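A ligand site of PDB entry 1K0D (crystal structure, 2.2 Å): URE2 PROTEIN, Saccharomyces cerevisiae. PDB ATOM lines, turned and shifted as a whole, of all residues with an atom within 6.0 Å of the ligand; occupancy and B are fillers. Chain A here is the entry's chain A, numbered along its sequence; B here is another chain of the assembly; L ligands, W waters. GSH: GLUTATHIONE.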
ATOM      1  N   HIS A  25      -3.908   6.104  10.416  1.00  0.00           N
ATOM      2  CA  HIS A  25      -3.172   5.190   9.558  1.00  0.00           C
ATOM      3  C   HIS A  25      -1.996   5.953   8.942  1.00  0.00           C
ATOM      4  O   HIS A  25      -2.059   7.179   8.768  1.00  0.00           O
ATOM      5  CB  HIS A  25      -4.081   4.636   8.464  1.00  0.00           C
ATOM      6  CG  HIS A  25      -3.394   3.680   7.537  1.00  0.00           C
ATOM      7  ND1 HIS A  25      -2.814   2.509   7.963  1.00  0.00           N
ATOM      8  CD2 HIS A  25      -3.217   3.723   6.196  1.00  0.00           C
ATOM      9  CE1 HIS A  25      -2.309   1.864   6.932  1.00  0.00           C
ATOM     10  NE2 HIS A  25      -2.536   2.575   5.842  1.00  0.00           N
ATOM     11  N   SER A  27      -0.916   6.286   5.914  1.00  0.00           N
ATOM     12  CA  SER A  27      -1.239   7.075   4.728  1.00  0.00           C
ATOM     13  C   SER A  27      -2.665   7.616   4.712  1.00  0.00           C
ATOM     14  O   SER A  27      -3.290   7.704   3.655  1.00  0.00           O
ATOM     15  CB  SER A  27      -0.999   6.242   3.458  1.00  0.00           C
ATOM     16  OG  SER A  27       0.386   6.001   3.250  1.00  0.00           O
ATOM     17  N   ALA A  28      -3.189   7.979   5.878  1.00  0.00           N
ATOM     18  CA  ALA A  28      -4.541   8.505   5.950  1.00  0.00           C
ATOM     19  C   ALA A  28      -4.524  10.029   6.048  1.00  0.00           C
ATOM     20  O   ALA A  28      -4.190  10.603   7.089  1.00  0.00           O
ATOM     21  CB  ALA A  28      -5.270   7.903   7.156  1.00  0.00           C
ATOM     22  N   PRO A  29      -4.864  10.717   4.949  1.00  0.00           N
ATOM     23  CA  PRO A  29      -4.870  12.186   4.986  1.00  0.00           C
ATOM     24  C   PRO A  29      -5.791  12.763   6.065  1.00  0.00           C
ATOM     25  O   PRO A  29      -5.468  13.787   6.659  1.00  0.00           O
ATOM     26  CB  PRO A  29      -5.327  12.551   3.570  1.00  0.00           C
ATOM     27  CG  PRO A  29      -4.718  11.449   2.742  1.00  0.00           C
ATOM     28  CD  PRO A  29      -5.046  10.222   3.573  1.00  0.00           C
ATOM     29  N   ASN A  30      -6.918  12.095   6.327  1.00  0.00           N
ATOM     30  CA  ASN A  30      -7.844  12.567   7.348  1.00  0.00           C
ATOM     31  C   ASN A  30      -7.261  12.431   8.735  1.00  0.00           C
ATOM     32  O   ASN A  30      -7.572  13.209   9.639  1.00  0.00           O
ATOM     33  CB  ASN A  30      -9.177  11.822   7.279  1.00  0.00           C
ATOM     34  CG  ASN A  30     -10.034  12.282   6.120  1.00  0.00           C
ATOM     35  OD1 ASN A  30     -10.242  13.481   5.915  1.00  0.00           O
ATOM     36  ND2 ASN A  30     -10.552  11.332   5.354  1.00  0.00           N
ATOM     37  N   GLY A  31      -6.411  11.415   8.920  1.00  0.00           N
ATOM     38  CA  GLY A  31      -5.781  11.209  10.208  1.00  0.00           C
ATOM     39  C   GLY A  31      -4.802  12.349  10.467  1.00  0.00           C
ATOM     40  O   GLY A  31      -4.768  12.886  11.563  1.00  0.00           O
ATOM     41  N   LYS A  33      -4.936  15.302   9.273  1.00  0.00           N
ATOM     42  CA  LYS A  33      -5.689  16.524   9.430  1.00  0.00           C
ATOM     43  C   LYS A  33      -5.898  16.791  10.926  1.00  0.00           C
ATOM     44  O   LYS A  33      -5.811  17.934  11.380  1.00  0.00           O
ATOM     45  CB  LYS A  33      -7.041  16.407   8.720  1.00  0.00           C
ATOM     46  CG  LYS A  33      -7.806  17.706   8.634  1.00  0.00           C
ATOM     47  CD  LYS A  33      -8.844  17.658   7.526  1.00  0.00           C
ATOM     48  CE  LYS A  33      -9.859  16.556   7.742  1.00  0.00           C
ATOM     49  NZ  LYS A  33     -10.815  16.523   6.614  1.00  0.00           N
ATOM     50  N   PHE A  52      -4.796  -1.810   8.569  1.00  0.00           N
ATOM     51  CA  PHE A  52      -6.006  -2.327   7.942  1.00  0.00           C
ATOM     52  C   PHE A  52      -5.755  -3.726   7.372  1.00  0.00           C
ATOM     53  O   PHE A  52      -6.646  -4.314   6.757  1.00  0.00           O
ATOM     54  CB  PHE A  52      -6.493  -1.380   6.856  1.00  0.00           C
ATOM     55  CG  PHE A  52      -6.728   0.029   7.342  1.00  0.00           C
ATOM     56  CD1 PHE A  52      -7.464   0.264   8.496  1.00  0.00           C
ATOM     57  CD2 PHE A  52      -6.213   1.118   6.627  1.00  0.00           C
ATOM     58  CE1 PHE A  52      -7.686   1.568   8.947  1.00  0.00           C
ATOM     59  CE2 PHE A  52      -6.435   2.422   7.078  1.00  0.00           C
ATOM     60  CZ  PHE A  52      -7.167   2.645   8.239  1.00  0.00           C
ATOM     61  N   HIS A  57      -9.165  -2.247  12.715  1.00  0.00           N
ATOM     62  CA  HIS A  57     -10.308  -1.343  12.724  1.00  0.00           C
ATOM     63  C   HIS A  57     -11.641  -2.095  12.817  1.00  0.00           C
ATOM     64  O   HIS A  57     -12.702  -1.480  12.874  1.00  0.00           O
ATOM     65  CB  HIS A  57     -10.275  -0.451  11.483  1.00  0.00           C
ATOM     66  CG  HIS A  57     -10.240  -1.204  10.184  1.00  0.00           C
ATOM     67  ND1 HIS A  57      -9.687  -2.458  10.066  1.00  0.00           N
ATOM     68  CD2 HIS A  57     -10.654  -0.863   8.950  1.00  0.00           C
ATOM     69  CE1 HIS A  57      -9.760  -2.858   8.810  1.00  0.00           C
ATOM     70  NE2 HIS A  57     -10.346  -1.908   8.105  1.00  0.00           N
ATOM     71  N   ASN A  68     -18.300   3.585  12.838  1.00  0.00           N
ATOM     72  CA  ASN A  68     -18.102   3.547  11.392  1.00  0.00           C
ATOM     73  C   ASN A  68     -16.861   2.729  11.045  1.00  0.00           C
ATOM     74  O   ASN A  68     -16.588   2.457   9.867  1.00  0.00           O
ATOM     75  CB  ASN A  68     -17.953   4.969  10.833  1.00  0.00           C
ATOM     76  CG  ASN A  68     -18.026   5.020   9.320  1.00  0.00           C
ATOM     77  OD1 ASN A  68     -17.406   5.862   8.688  1.00  0.00           O
ATOM     78  ND2 ASN A  68     -18.792   4.107   8.738  1.00  0.00           N
ATOM     79  N   ALA A  69     -16.104   2.336  12.057  1.00  0.00           N
ATOM     80  CA  ALA A  69     -14.898   1.533  11.871  1.00  0.00           C
ATOM     81  C   ALA A  69     -13.918   2.150  10.881  1.00  0.00           C
ATOM     82  O   ALA A  69     -13.358   1.459  10.032  1.00  0.00           O
ATOM     83  CB  ALA A  69     -15.273   0.119  11.413  1.00  0.00           C
ATOM     84  N   ARG A  70     -13.716   3.461  11.000  1.00  0.00           N
ATOM     85  CA  ARG A  70     -12.796   4.173  10.119  1.00  0.00           C
ATOM     86  C   ARG A  70     -11.904   5.113  10.934  1.00  0.00           C
ATOM     87  O   ARG A  70     -12.142   5.362  12.112  1.00  0.00           O
ATOM     88  CB  ARG A  70     -13.593   4.982   9.105  1.00  0.00           C
ATOM     89  CG  ARG A  70     -14.421   4.152   8.131  1.00  0.00           C
ATOM     90  CD  ARG A  70     -13.548   3.581   7.027  1.00  0.00           C
ATOM     91  NE  ARG A  70     -14.293   2.733   6.096  1.00  0.00           N
ATOM     92  CZ  ARG A  70     -14.743   1.514   6.393  1.00  0.00           C
ATOM     93  NH1 ARG A  70     -14.500   0.975   7.584  1.00  0.00           N
ATOM     94  NH2 ARG A  70     -15.413   0.822   5.482  1.00  0.00           N
ATOM     95  N   VAL A  71     -10.841   5.603  10.303  1.00  0.00           N
ATOM     96  CA  VAL A  71      -9.959   6.543  10.982  1.00  0.00           C
ATOM     97  C   VAL A  71     -10.161   7.881  10.277  1.00  0.00           C
ATOM     98  O   VAL A  71     -10.462   7.919   9.076  1.00  0.00           O
ATOM     99  CB  VAL A  71      -8.467   6.108  10.908  1.00  0.00           C
ATOM    100  CG1 VAL A  71      -8.260   4.837  11.725  1.00  0.00           C
ATOM    101  CG2 VAL A  71      -8.055   5.882   9.469  1.00  0.00           C
ATOM    102  N   PRO A  72      -9.979   8.986  10.998  1.00  0.00           N
ATOM    103  CA  PRO A  72      -9.588   9.050  12.405  1.00  0.00           C
ATOM    104  C   PRO A  72     -10.683   8.894  13.460  1.00  0.00           C
ATOM    105  O   PRO A  72     -11.880   9.015  13.200  1.00  0.00           O
ATOM    106  CB  PRO A  72      -8.930  10.408  12.508  1.00  0.00           C
ATOM    107  CG  PRO A  72      -9.818  11.237  11.620  1.00  0.00           C
ATOM    108  CD  PRO A  72     -10.017  10.342  10.406  1.00  0.00           C
ATOM    109  N   TRP A  85     -15.421  10.627  16.616  1.00  0.00           N
ATOM    110  CA  TRP A  85     -15.049  10.136  15.292  1.00  0.00           C
ATOM    111  C   TRP A  85     -15.517  11.123  14.207  1.00  0.00           C
ATOM    112  O   TRP A  85     -16.378  11.960  14.463  1.00  0.00           O
ATOM    113  CB  TRP A  85     -15.643   8.747  15.058  1.00  0.00           C
ATOM    114  CG  TRP A  85     -17.083   8.632  15.440  1.00  0.00           C
ATOM    115  CD1 TRP A  85     -17.599   8.677  16.703  1.00  0.00           C
ATOM    116  CD2 TRP A  85     -18.187   8.458  14.555  1.00  0.00           C
ATOM    117  NE1 TRP A  85     -18.963   8.537  16.658  1.00  0.00           N
ATOM    118  CE2 TRP A  85     -19.352   8.398  15.358  1.00  0.00           C
ATOM    119  CE3 TRP A  85     -18.322   8.340  13.163  1.00  0.00           C
ATOM    120  CZ2 TRP A  85     -20.629   8.241  14.814  1.00  0.00           C
ATOM    121  CZ3 TRP A  85     -19.591   8.178  12.622  1.00  0.00           C
ATOM    122  CH2 TRP A  85     -20.733   8.126  13.443  1.00  0.00           C
ATOM    123  N   GLU A  86     -14.944  10.997  13.007  1.00  0.00           N
ATOM    124  CA  GLU A  86     -15.222  11.897  11.865  1.00  0.00           C
ATOM    125  C   GLU A  86     -14.310  13.103  12.069  1.00  0.00           C
ATOM    126  O   GLU A  86     -14.467  13.851  13.033  1.00  0.00           O
ATOM    127  CB  GLU A  86     -16.684  12.352  11.816  1.00  0.00           C
ATOM    128  CG  GLU A  86     -17.626  11.318  11.230  1.00  0.00           C
ATOM    129  CD  GLU A  86     -17.339  11.016   9.763  1.00  0.00           C
ATOM    130  OE1 GLU A  86     -17.470   9.837   9.362  1.00  0.00           O
ATOM    131  OE2 GLU A  86     -16.998  11.944   8.998  1.00  0.00           O
ATOM    132  N   SER A  87     -13.352  13.267  11.157  1.00  0.00           N
ATOM    133  CA  SER A  87     -12.391  14.348  11.233  1.00  0.00           C
ATOM    134  C   SER A  87     -13.016  15.719  11.459  1.00  0.00           C
ATOM    135  O   SER A  87     -12.508  16.507  12.253  1.00  0.00           O
ATOM    136  CB  SER A  87     -11.514  14.352   9.965  1.00  0.00           C
ATOM    137  OG  SER A  87     -12.261  14.687   8.803  1.00  0.00           O
ATOM    138  N   GLY A  88     -14.127  15.991  10.771  1.00  0.00           N
ATOM    139  CA  GLY A  88     -14.800  17.278  10.928  1.00  0.00           C
ATOM    140  C   GLY A  88     -15.271  17.554  12.342  1.00  0.00           C
ATOM    141  O   GLY A  88     -15.116  18.666  12.868  1.00  0.00           O
ATOM    142  N   THR A 126     -14.801  18.167   3.728  1.00  0.00           N
ATOM    143  CA  THR A 126     -15.091  16.788   4.118  1.00  0.00           C
ATOM    144  C   THR A 126     -16.141  16.069   3.280  1.00  0.00           C
ATOM    145  O   THR A 126     -16.102  14.843   3.150  1.00  0.00           O
ATOM    146  CB  THR A 126     -15.570  16.700   5.597  1.00  0.00           C
ATOM    147  OG1 THR A 126     -16.808  17.396   5.738  1.00  0.00           O
ATOM    148  CG2 THR A 126     -14.544  17.348   6.519  1.00  0.00           C
ATOM    149  N   TRP A 222      -4.833  16.706   1.894  1.00  0.00           N
ATOM    150  CA  TRP A 222      -5.339  16.239   0.618  1.00  0.00           C
ATOM    151  C   TRP A 222      -4.727  16.934  -0.579  1.00  0.00           C
ATOM    152  O   TRP A 222      -4.556  16.322  -1.637  1.00  0.00           O
ATOM    153  CB  TRP A 222      -6.868  16.362   0.573  1.00  0.00           C
ATOM    154  CG  TRP A 222      -7.539  15.397   1.505  1.00  0.00           C
ATOM    155  CD1 TRP A 222      -7.945  15.641   2.788  1.00  0.00           C
ATOM    156  CD2 TRP A 222      -7.835  14.030   1.236  1.00  0.00           C
ATOM    157  NE1 TRP A 222      -8.486  14.507   3.335  1.00  0.00           N
ATOM    158  CE2 TRP A 222      -8.424  13.500   2.404  1.00  0.00           C
ATOM    159  CE3 TRP A 222      -7.661  13.194   0.126  1.00  0.00           C
ATOM    160  CZ2 TRP A 222      -8.853  12.169   2.489  1.00  0.00           C
ATOM    161  CZ3 TRP A 222      -8.085  11.875   0.215  1.00  0.00           C
ATOM    162  CH2 TRP A 222      -8.668  11.382   1.387  1.00  0.00           C
ATOM    163  N   PHE B 123     -21.530  14.860  10.513  1.00  0.00           N
ATOM    164  CA  PHE B 123     -20.463  14.768   9.519  1.00  0.00           C
ATOM    165  C   PHE B 123     -20.529  13.408   8.828  1.00  0.00           C
ATOM    166  O   PHE B 123     -20.278  13.304   7.620  1.00  0.00           O
ATOM    167  CB  PHE B 123     -19.090  15.003  10.157  1.00  0.00           C
ATOM    168  CG  PHE B 123     -18.649  16.449  10.159  1.00  0.00           C
ATOM    169  CD1 PHE B 123     -18.816  17.240  11.293  1.00  0.00           C
ATOM    170  CD2 PHE B 123     -18.097  17.027   9.011  1.00  0.00           C
ATOM    171  CE1 PHE B 123     -18.438  18.588  11.301  1.00  0.00           C
ATOM    172  CE2 PHE B 123     -17.715  18.373   8.998  1.00  0.00           C
ATOM    173  CZ  PHE B 123     -17.892  19.154  10.148  1.00  0.00           C
ATOM    174  N   SER B 127     -20.999  13.498   4.851  1.00  0.00           N
ATOM    175  CA  SER B 127     -19.795  13.023   4.169  1.00  0.00           C
ATOM    176  C   SER B 127     -19.736  11.552   3.794  1.00  0.00           C
ATOM    177  O   SER B 127     -19.113  11.197   2.792  1.00  0.00           O
ATOM    178  CB  SER B 127     -18.559  13.383   5.001  1.00  0.00           C
ATOM    179  OG  SER B 127     -18.571  14.778   5.313  1.00  0.00           O
ATOM    180  N   GLY B 128     -20.367  10.678   4.577  1.00  0.00           N
ATOM    181  CA  GLY B 128     -20.320   9.261   4.265  1.00  0.00           C
ATOM    182  C   GLY B 128     -21.605   8.631   3.753  1.00  0.00           C
ATOM    183  O   GLY B 128     -21.583   7.597   3.096  1.00  0.00           O
HETATM  184  N1  GSH L   1     -15.541  11.327   6.416  1.00  0.00           N
HETATM  185  CA1 GSH L   1     -14.531  10.646   7.216  1.00  0.00           C
HETATM  186  C1  GSH L   1     -13.650  11.636   8.039  1.00  0.00           C
HETATM  187  O11 GSH L   1     -13.559  12.809   7.654  1.00  0.00           O
HETATM  188  O12 GSH L   1     -13.042  11.156   9.096  1.00  0.00           O
HETATM  189  CB1 GSH L   1     -13.648   9.757   6.288  1.00  0.00           C
HETATM  190  CG1 GSH L   1     -13.148   8.491   7.055  1.00  0.00           C
HETATM  191  CD1 GSH L   1     -12.259   7.614   6.132  1.00  0.00           C
HETATM  192  OE1 GSH L   1     -12.724   7.101   5.094  1.00  0.00           O
HETATM  193  N2  GSH L   1     -10.988   7.458   6.568  1.00  0.00           N
HETATM  194  CA2 GSH L   1     -10.025   6.631   5.809  1.00  0.00           C
HETATM  195  C2  GSH L   1     -10.081   5.161   6.314  1.00  0.00           C
HETATM  196  O2  GSH L   1     -10.317   4.878   7.499  1.00  0.00           O
HETATM  197  CB2 GSH L   1      -8.584   7.186   6.022  1.00  0.00           C
HETATM  198  SG2 GSH L   1      -8.343   8.852   5.325  1.00  0.00           S
HETATM  199  N3  GSH L   1      -9.833   4.200   5.381  1.00  0.00           N
HETATM  200  CA3 GSH L   1      -9.834   2.751   5.672  1.00  0.00           C
HETATM  201  C3  GSH L   1     -10.978   2.055   4.934  1.00  0.00           C
HETATM  202  O31 GSH L   1     -11.067   0.825   5.111  1.00  0.00           O
HETATM  203  O32 GSH L   1     -11.753   2.735   4.201  1.00  0.00           O
HETATM  204  O   HOH W   1     -14.584  13.189   4.340  1.00  0.00           O
HETATM  205  O   HOH W   2     -15.417  14.355   8.877  1.00  0.00           O
HETATM  206  O   HOH W   3     -17.794   9.277   6.815  1.00  0.00           O
HETATM  207  O   HOH W   4     -13.371   8.906  11.010  1.00  0.00           O
HETATM  208  O   HOH W   5     -16.335  10.167   4.002  1.00  0.00           O
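Water W2 lies within hydrogen-bond range of an oxygen (O11) of the ligand, the backbone NH of Gly 88, the side-chain carboxylate of Glu 86 and the side-chain hydroxyl of Ser 87. Water W5 bridges N1 of the ligand (2.8 Å) and O of Ser 127 of chain B (3.2 Å). Water W1 lies within hydrogen-bond range of O of Thr 126 (2.5 Å) and N1 of the ligand (2.9 Å). Water W4 lies within hydrogen-bond range of the backbone carbonyl oxygen (O) of Pro 72 (2.7 Å), an oxygen (O12) of the ligand (3.0 Å) and the backbone NH (N) of Glu 86 (3.3 Å). Water W3 lies within hydrogen-bond range of OE1 of Glu 86 (2.6 Å) and N1 of the ligand (3.1 Å).
An oxygen (O12) of the ligand sits at hydrogen-bond distance from the backbone NH (N) of Ser 87, 3.0 Å away. OG of Ser 87 lies within hydrogen-bond range of O11 of the ligand, at 2.6 Å. N of Val 71 lies within hydrogen-bond range of O2 of the ligand, at 2.9 Å. A nitrogen (N2) of the ligand lies within hydrogen-bond range of the backbone carbonyl oxygen (O) of Val 71 (2.6 Å). A nitrogen (N1) of the ligand is in salt-bridge range of the side-chain carboxylate (OE2) of Glu 86 (3.0 Å). NE of Arg 70 is in salt-bridge range of O32 of the ligand. The backbone NH of Asn 30 sits close to a sulfur (SG2) of the ligand (3.7 Å). A sulfur (SG2) of the ligand lies close to the side-chain amide nitrogen of Asn 30 (3.3 Å).
CB of Ala 28 touches CB2 of the ligand, 3.6 Å away. Pro 29 touches the ligand (N to SG2, 3.97 Å). Phe 52 touches the ligand (CE2 to CA3, 3.7 Å). Pro 72 touches the ligand (CD to O12, 3.4 Å). CB of Ser 127 of chain B touches N1 of the ligand (3.9 Å). Hydrophobic or aromatic side chains that line the ligand: Ala 28, Pro 29, Phe 52, Val 71 and Pro 72. Within 4 Å of the ligand: Ala 28, Pro 29, Asn 30, Phe 52, Arg 70, Val 71, Pro 72, Glu 86, Ser 87 and Ser 127 of chain B. The nearest printed residue that does not touch the ligand is His 57 (4.1 Å).
The side-chain hydroxyl (OG) of Ser 87 sits at hydrogen-bond distance from the side-chain amino group (NZ) of Lys 33 (3.2 Å). NH1 of Arg 70 sits close to O of Asn 68. NE1 of Trp 222 lies within hydrogen-bond range of OD1 of Asn 30 (3.3 Å). The side-chain amino group of Lys 33 is in hydrogen-bond range of the side-chain amide oxygen of Asn 30 (3.2 Å). The side-chain hydroxyl (OG) of Ser 127 of chain B sits at hydrogen-bond distance from the side-chain hydroxyl (OG1) of Thr 126. The side-chain hydroxyl (OG) of Ser 127 of chain B sits close to the backbone carbonyl oxygen (O) of Phe 123 of chain B (3.2 Å).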
